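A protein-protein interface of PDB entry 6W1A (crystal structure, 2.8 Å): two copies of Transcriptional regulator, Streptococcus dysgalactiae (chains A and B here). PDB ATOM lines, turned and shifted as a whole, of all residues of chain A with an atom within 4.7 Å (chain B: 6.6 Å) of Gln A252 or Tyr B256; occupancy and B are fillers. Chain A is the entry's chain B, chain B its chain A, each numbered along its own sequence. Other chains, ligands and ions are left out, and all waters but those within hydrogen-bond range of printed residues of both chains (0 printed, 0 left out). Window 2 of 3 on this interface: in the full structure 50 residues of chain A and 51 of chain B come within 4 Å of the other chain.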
ATOM      1  N   LEU A 228     -36.525  22.928   6.971  1.00  0.00           N
ATOM      2  CA  LEU A 228     -35.870  23.873   7.869  1.00  0.00           C
ATOM      3  C   LEU A 228     -35.697  25.231   7.206  1.00  0.00           C
ATOM      4  O   LEU A 228     -35.949  26.272   7.825  1.00  0.00           O
ATOM      5  CB  LEU A 228     -34.517  23.318   8.314  1.00  0.00           C
ATOM      6  CG  LEU A 228     -33.598  24.264   9.088  1.00  0.00           C
ATOM      7  CD1 LEU A 228     -34.105  24.492  10.507  1.00  0.00           C
ATOM      8  CD2 LEU A 228     -32.184  23.709   9.102  1.00  0.00           C
ATOM      9  N   ARG A 248     -30.110  29.847   7.209  1.00  0.00           N
ATOM     10  CA  ARG A 248     -28.659  29.808   7.083  1.00  0.00           C
ATOM     11  C   ARG A 248     -28.095  28.463   7.518  1.00  0.00           C
ATOM     12  O   ARG A 248     -27.111  27.992   6.938  1.00  0.00           O
ATOM     13  CB  ARG A 248     -28.042  30.937   7.915  1.00  0.00           C
ATOM     14  CG  ARG A 248     -26.634  31.345   7.515  1.00  0.00           C
ATOM     15  CD  ARG A 248     -25.579  30.620   8.338  1.00  0.00           C
ATOM     16  NE  ARG A 248     -24.272  31.265   8.237  1.00  0.00           N
ATOM     17  CZ  ARG A 248     -23.429  31.091   7.224  1.00  0.00           C
ATOM     18  NH1 ARG A 248     -22.262  31.721   7.217  1.00  0.00           N
ATOM     19  NH2 ARG A 248     -23.753  30.293   6.215  1.00  0.00           N
ATOM     20  N   GLN A 249     -28.722  27.821   8.507  1.00  0.00           N
ATOM     21  CA  GLN A 249     -28.328  26.469   8.883  1.00  0.00           C
ATOM     22  C   GLN A 249     -28.622  25.483   7.760  1.00  0.00           C
ATOM     23  O   GLN A 249     -27.838  24.556   7.520  1.00  0.00           O
ATOM     24  CB  GLN A 249     -29.040  26.057  10.174  1.00  0.00           C
ATOM     25  CG  GLN A 249     -28.559  26.811  11.406  1.00  0.00           C
ATOM     26  CD  GLN A 249     -29.381  26.511  12.647  1.00  0.00           C
ATOM     27  OE1 GLN A 249     -30.468  25.936  12.568  1.00  0.00           O
ATOM     28  NE2 GLN A 249     -28.865  26.909  13.803  1.00  0.00           N
ATOM     29  N   ALA A 250     -29.737  25.675   7.052  1.00  0.00           N
ATOM     30  CA  ALA A 250     -30.063  24.801   5.931  1.00  0.00           C
ATOM     31  C   ALA A 250     -29.043  24.935   4.809  1.00  0.00           C
ATOM     32  O   ALA A 250     -28.673  23.939   4.177  1.00  0.00           O
ATOM     33  CB  ALA A 250     -31.470  25.106   5.418  1.00  0.00           C
ATOM     34  N   LEU A 251     -28.573  26.156   4.545  1.00  0.00           N
ATOM     35  CA  LEU A 251     -27.550  26.343   3.522  1.00  0.00           C
ATOM     36  C   LEU A 251     -26.259  25.626   3.901  1.00  0.00           C
ATOM     37  O   LEU A 251     -25.588  25.042   3.041  1.00  0.00           O
ATOM     38  CB  LEU A 251     -27.296  27.833   3.292  1.00  0.00           C
ATOM     39  CG  LEU A 251     -28.431  28.605   2.608  1.00  0.00           C
ATOM     40  CD1 LEU A 251     -28.150  30.103   2.585  1.00  0.00           C
ATOM     41  CD2 LEU A 251     -28.676  28.084   1.200  1.00  0.00           C
ATOM     42  N   GLN A 252     -25.908  25.630   5.190  1.00  0.00           N
ATOM     43  CA  GLN A 252     -24.686  24.946   5.605  1.00  0.00           C
ATOM     44  C   GLN A 252     -24.820  23.436   5.497  1.00  0.00           C
ATOM     45  O   GLN A 252     -23.817  22.742   5.300  1.00  0.00           O
ATOM     46  CB  GLN A 252     -24.316  25.328   7.036  1.00  0.00           C
ATOM     47  CG  GLN A 252     -24.224  26.817   7.284  1.00  0.00           C
ATOM     48  CD  GLN A 252     -23.164  27.162   8.309  1.00  0.00           C
ATOM     49  OE1 GLN A 252     -23.436  27.212   9.509  1.00  0.00           O
ATOM     50  NE2 GLN A 252     -21.944  27.403   7.839  1.00  0.00           N
ATOM     51  N   ILE A 253     -26.037  22.907   5.615  1.00  0.00           N
ATOM     52  CA  ILE A 253     -26.236  21.477   5.412  1.00  0.00           C
ATOM     53  C   ILE A 253     -25.970  21.107   3.958  1.00  0.00           C
ATOM     54  O   ILE A 253     -25.272  20.128   3.665  1.00  0.00           O
ATOM     55  CB  ILE A 253     -27.647  21.070   5.864  1.00  0.00           C
ATOM     56  CG1 ILE A 253     -27.776  21.259   7.380  1.00  0.00           C
ATOM     57  CG2 ILE A 253     -27.946  19.627   5.459  1.00  0.00           C
ATOM     58  CD1 ILE A 253     -29.197  21.164   7.912  1.00  0.00           C
ATOM     59  N   PHE A 254     -26.505  21.898   3.023  1.00  0.00           N
ATOM     60  CA  PHE A 254     -26.177  21.700   1.614  1.00  0.00           C
ATOM     61  C   PHE A 254     -24.684  21.858   1.369  1.00  0.00           C
ATOM     62  O   PHE A 254     -24.093  21.111   0.581  1.00  0.00           O
ATOM     63  CB  PHE A 254     -26.960  22.687   0.752  1.00  0.00           C
ATOM     64  CG  PHE A 254     -28.439  22.448   0.747  1.00  0.00           C
ATOM     65  CD1 PHE A 254     -29.324  23.499   0.910  1.00  0.00           C
ATOM     66  CD2 PHE A 254     -28.945  21.172   0.569  1.00  0.00           C
ATOM     67  CE1 PHE A 254     -30.686  23.282   0.903  1.00  0.00           C
ATOM     68  CE2 PHE A 254     -30.307  20.949   0.557  1.00  0.00           C
ATOM     69  CZ  PHE A 254     -31.178  22.003   0.726  1.00  0.00           C
ATOM     70  N   LYS A 255     -24.054  22.824   2.043  1.00  0.00           N
ATOM     71  CA  LYS A 255     -22.623  23.040   1.866  1.00  0.00           C
ATOM     72  C   LYS A 255     -21.820  21.871   2.422  1.00  0.00           C
ATOM     73  O   LYS A 255     -20.899  21.377   1.763  1.00  0.00           O
ATOM     74  CB  LYS A 255     -22.199  24.350   2.535  1.00  0.00           C
ATOM     75  CG  LYS A 255     -20.736  24.719   2.317  1.00  0.00           C
ATOM     76  CD  LYS A 255     -20.245  25.743   3.335  1.00  0.00           C
ATOM     77  CE  LYS A 255     -20.513  27.171   2.880  1.00  0.00           C
ATOM     78  NZ  LYS A 255     -20.680  28.112   4.027  1.00  0.00           N
ATOM     79  N   TYR A 256     -22.166  21.405   3.623  1.00  0.00           N
ATOM     80  CA  TYR A 256     -21.387  20.347   4.255  1.00  0.00           C
ATOM     81  C   TYR A 256     -21.538  19.021   3.522  1.00  0.00           C
ATOM     82  O   TYR A 256     -20.652  18.166   3.608  1.00  0.00           O
ATOM     83  CB  TYR A 256     -21.791  20.183   5.721  1.00  0.00           C
ATOM     84  CG  TYR A 256     -21.523  21.396   6.582  1.00  0.00           C
ATOM     85  CD1 TYR A 256     -22.169  21.562   7.802  1.00  0.00           C
ATOM     86  CD2 TYR A 256     -20.629  22.382   6.173  1.00  0.00           C
ATOM     87  CE1 TYR A 256     -21.931  22.675   8.590  1.00  0.00           C
ATOM     88  CE2 TYR A 256     -20.386  23.497   6.953  1.00  0.00           C
ATOM     89  CZ  TYR A 256     -21.038  23.638   8.159  1.00  0.00           C
ATOM     90  OH  TYR A 256     -20.793  24.746   8.934  1.00  0.00           O
ATOM     91  N   GLN B 249     -18.711  19.082  11.115  1.00  0.00           N
ATOM     92  CA  GLN B 249     -19.767  19.562  10.229  1.00  0.00           C
ATOM     93  C   GLN B 249     -20.966  18.622  10.252  1.00  0.00           C
ATOM     94  O   GLN B 249     -22.118  19.071  10.199  1.00  0.00           O
ATOM     95  CB  GLN B 249     -19.243  19.708   8.802  1.00  0.00           C
ATOM     96  CG  GLN B 249     -18.275  20.853   8.589  1.00  0.00           C
ATOM     97  CD  GLN B 249     -17.755  20.902   7.168  1.00  0.00           C
ATOM     98  OE1 GLN B 249     -17.905  19.946   6.406  1.00  0.00           O
ATOM     99  NE2 GLN B 249     -17.140  22.015   6.802  1.00  0.00           N
ATOM    100  N   LEU B 251     -21.788  16.772  12.857  1.00  0.00           N
ATOM    101  CA  LEU B 251     -22.416  16.983  14.157  1.00  0.00           C
ATOM    102  C   LEU B 251     -23.311  18.214  14.142  1.00  0.00           C
ATOM    103  O   LEU B 251     -24.383  18.218  14.757  1.00  0.00           O
ATOM    104  CB  LEU B 251     -21.350  17.111  15.244  1.00  0.00           C
ATOM    105  CG  LEU B 251     -20.607  15.835  15.643  1.00  0.00           C
ATOM    106  CD1 LEU B 251     -19.546  16.138  16.690  1.00  0.00           C
ATOM    107  CD2 LEU B 251     -21.585  14.783  16.149  1.00  0.00           C
ATOM    108  N   GLN B 252     -22.892  19.274  13.442  1.00  0.00           N
ATOM    109  CA  GLN B 252     -23.731  20.465  13.382  1.00  0.00           C
ATOM    110  C   GLN B 252     -24.971  20.223  12.534  1.00  0.00           C
ATOM    111  O   GLN B 252     -26.011  20.848  12.769  1.00  0.00           O
ATOM    112  CB  GLN B 252     -22.940  21.661  12.848  1.00  0.00           C
ATOM    113  CG  GLN B 252     -21.611  21.903  13.550  1.00  0.00           C
ATOM    114  CD  GLN B 252     -21.771  22.362  14.990  1.00  0.00           C
ATOM    115  OE1 GLN B 252     -21.608  21.577  15.926  1.00  0.00           O
ATOM    116  NE2 GLN B 252     -22.084  23.640  15.174  1.00  0.00           N
ATOM    117  N   ILE B 253     -24.892  19.308  11.565  1.00  0.00           N
ATOM    118  CA  ILE B 253     -26.086  18.937  10.814  1.00  0.00           C
ATOM    119  C   ILE B 253     -27.085  18.252  11.733  1.00  0.00           C
ATOM    120  O   ILE B 253     -28.288  18.542  11.693  1.00  0.00           O
ATOM    121  CB  ILE B 253     -25.718  18.048   9.611  1.00  0.00           C
ATOM    122  CG1 ILE B 253     -24.892  18.830   8.590  1.00  0.00           C
ATOM    123  CG2 ILE B 253     -26.976  17.499   8.942  1.00  0.00           C
ATOM    124  CD1 ILE B 253     -24.289  17.953   7.510  1.00  0.00           C
ATOM    125  N   PHE B 254     -26.604  17.341  12.584  1.00  0.00           N
ATOM    126  CA  PHE B 254     -27.469  16.754  13.599  1.00  0.00           C
ATOM    127  C   PHE B 254     -28.048  17.831  14.507  1.00  0.00           C
ATOM    128  O   PHE B 254     -29.222  17.767  14.891  1.00  0.00           O
ATOM    129  CB  PHE B 254     -26.692  15.732  14.423  1.00  0.00           C
ATOM    130  CG  PHE B 254     -26.286  14.514  13.649  1.00  0.00           C
ATOM    131  CD1 PHE B 254     -27.069  14.044  12.605  1.00  0.00           C
ATOM    132  CD2 PHE B 254     -25.120  13.834  13.967  1.00  0.00           C
ATOM    133  CE1 PHE B 254     -26.699  12.918  11.894  1.00  0.00           C
ATOM    134  CE2 PHE B 254     -24.742  12.712  13.257  1.00  0.00           C
ATOM    135  CZ  PHE B 254     -25.534  12.252  12.220  1.00  0.00           C
ATOM    136  N   LYS B 255     -27.240  18.842  14.841  1.00  0.00           N
ATOM    137  CA  LYS B 255     -27.709  19.920  15.703  1.00  0.00           C
ATOM    138  C   LYS B 255     -28.780  20.756  15.013  1.00  0.00           C
ATOM    139  O   LYS B 255     -29.825  21.046  15.608  1.00  0.00           O
ATOM    140  CB  LYS B 255     -26.531  20.800  16.124  1.00  0.00           C
ATOM    141  CG  LYS B 255     -26.883  21.912  17.104  1.00  0.00           C
ATOM    142  CD  LYS B 255     -25.673  22.787  17.405  1.00  0.00           C
ATOM    143  CE  LYS B 255     -24.525  21.978  17.997  1.00  0.00           C
ATOM    144  NZ  LYS B 255     -23.865  22.692  19.128  1.00  0.00           N
ATOM    145  N   TYR B 256     -28.553  21.127  13.748  1.00  0.00           N
ATOM    146  CA  TYR B 256     -29.489  22.016  13.067  1.00  0.00           C
ATOM    147  C   TYR B 256     -30.824  21.332  12.789  1.00  0.00           C
ATOM    148  O   TYR B 256     -31.855  22.008  12.695  1.00  0.00           O
ATOM    149  CB  TYR B 256     -28.889  22.522  11.751  1.00  0.00           C
ATOM    150  CG  TYR B 256     -27.588  23.293  11.872  1.00  0.00           C
ATOM    151  CD1 TYR B 256     -27.197  23.871  13.073  1.00  0.00           C
ATOM    152  CD2 TYR B 256     -26.744  23.432  10.776  1.00  0.00           C
ATOM    153  CE1 TYR B 256     -26.002  24.571  13.175  1.00  0.00           C
ATOM    154  CE2 TYR B 256     -25.552  24.125  10.868  1.00  0.00           C
ATOM    155  CZ  TYR B 256     -25.185  24.694  12.068  1.00  0.00           C
ATOM    156  OH  TYR B 256     -23.996  25.384  12.150  1.00  0.00           O
ATOM    157  N   LEU B 257     -30.834  20.008  12.665  1.00  0.00           N
ATOM    158  CA  LEU B 257     -32.046  19.269  12.339  1.00  0.00           C
ATOM    159  C   LEU B 257     -32.732  18.680  13.563  1.00  0.00           C
ATOM    160  O   LEU B 257     -33.664  17.883  13.413  1.00  0.00           O
ATOM    161  CB  LEU B 257     -31.734  18.164  11.329  1.00  0.00           C
ATOM    162  CG  LEU B 257     -31.280  18.648   9.949  1.00  0.00           C
ATOM    163  CD1 LEU B 257     -30.924  17.471   9.057  1.00  0.00           C
ATOM    164  CD2 LEU B 257     -32.346  19.518   9.293  1.00  0.00           C
ATOM    165  N   GLY B 258     -32.295  19.048  14.768  1.00  0.00           N
ATOM    166  CA  GLY B 258     -32.928  18.576  15.983  1.00  0.00           C
ATOM    167  C   GLY B 258     -32.747  17.109  16.298  1.00  0.00           C
ATOM    168  O   GLY B 258     -33.411  16.603  17.206  1.00  0.00           O
ATOM    169  N   GLU B 259     -31.875  16.404  15.575  1.00  0.00           N
ATOM    170  CA  GLU B 259     -31.621  14.985  15.825  1.00  0.00           C
ATOM    171  C   GLU B 259     -30.699  14.853  17.033  1.00  0.00           C
ATOM    172  O   GLU B 259     -29.487  14.650  16.920  1.00  0.00           O
ATOM    173  CB  GLU B 259     -31.032  14.318  14.589  1.00  0.00           C
ATOM    174  CG  GLU B 259     -31.926  14.406  13.362  1.00  0.00           C
ATOM    175  CD  GLU B 259     -33.187  13.573  13.501  1.00  0.00           C
ATOM    176  OE1 GLU B 259     -33.070  12.359  13.769  1.00  0.00           O
ATOM    177  OE2 GLU B 259     -34.295  14.137  13.349  1.00  0.00           O
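NE2 of Gln A252 sits at hydrogen-bond distance from OH of Tyr A256 (3.1 Å).
Of the 10 printed residues of chain B, 4 touch a printed residue of chain A. Of the 10 printed residues of chain A, 5 touch a printed residue of chain B. Printed residues of chain A that touch a printed residue of chain B: Leu A228, Gln A249, Gln A252, Ile A253 and Tyr A256. Among the printed residues, 7 pairs touch across the chains.
Gln A249 touches Tyr B256, and with the chains exchanged Tyr A256 touches Gln B249. Gln A252 touches Tyr B256, but with the chains exchanged Tyr A256 does not touch Gln B252 (4.5 Å). Ile A253 touches its own counterpart, Ile B253. Tyr A256 touches Ile B253, but with the chains exchanged Ile A253 does not touch Tyr B256 (4.1 Å). 7 positions are printed for both chains. Of the 7 pairs that touch across the chains among the printed residues, 3 have their exchanged pair printed and touching as well.
The side-chain hydroxyl (OH) of Tyr B256 sits at hydrogen-bond distance from the side-chain amide oxygen (OE1) of Gln A252 (3.3 Å).
Tyr B256 touches Leu A228 (O to CD2, 3.99 Å). CD of Gln A249 touches CD1 of Tyr B256 (3.5 Å). Ile B253 touches Ile A253. Leu B257 touches Ile A253. Tyr A256 touches Gln B249 (CD2 to CD, 3.4 Å). Tyr A256 touches Ile B253 (CB to CD1, 3.8 Å).
Of the printed residues of chain A, Tyr B256 touches Leu A228, Gln A249 and Gln A252. Printed residues of chain A within 4 Å of Ile B253: Ile A253 (3.96 Å) and Tyr A256 (3.8 Å). Of the printed residues of chain B, Tyr A256 touches Gln B249 (3.4 Å) and Ile B253 (3.8 Å). The nearest printed residue of chain A that does not touch Tyr B256 is Ile A253 (4.1 Å).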
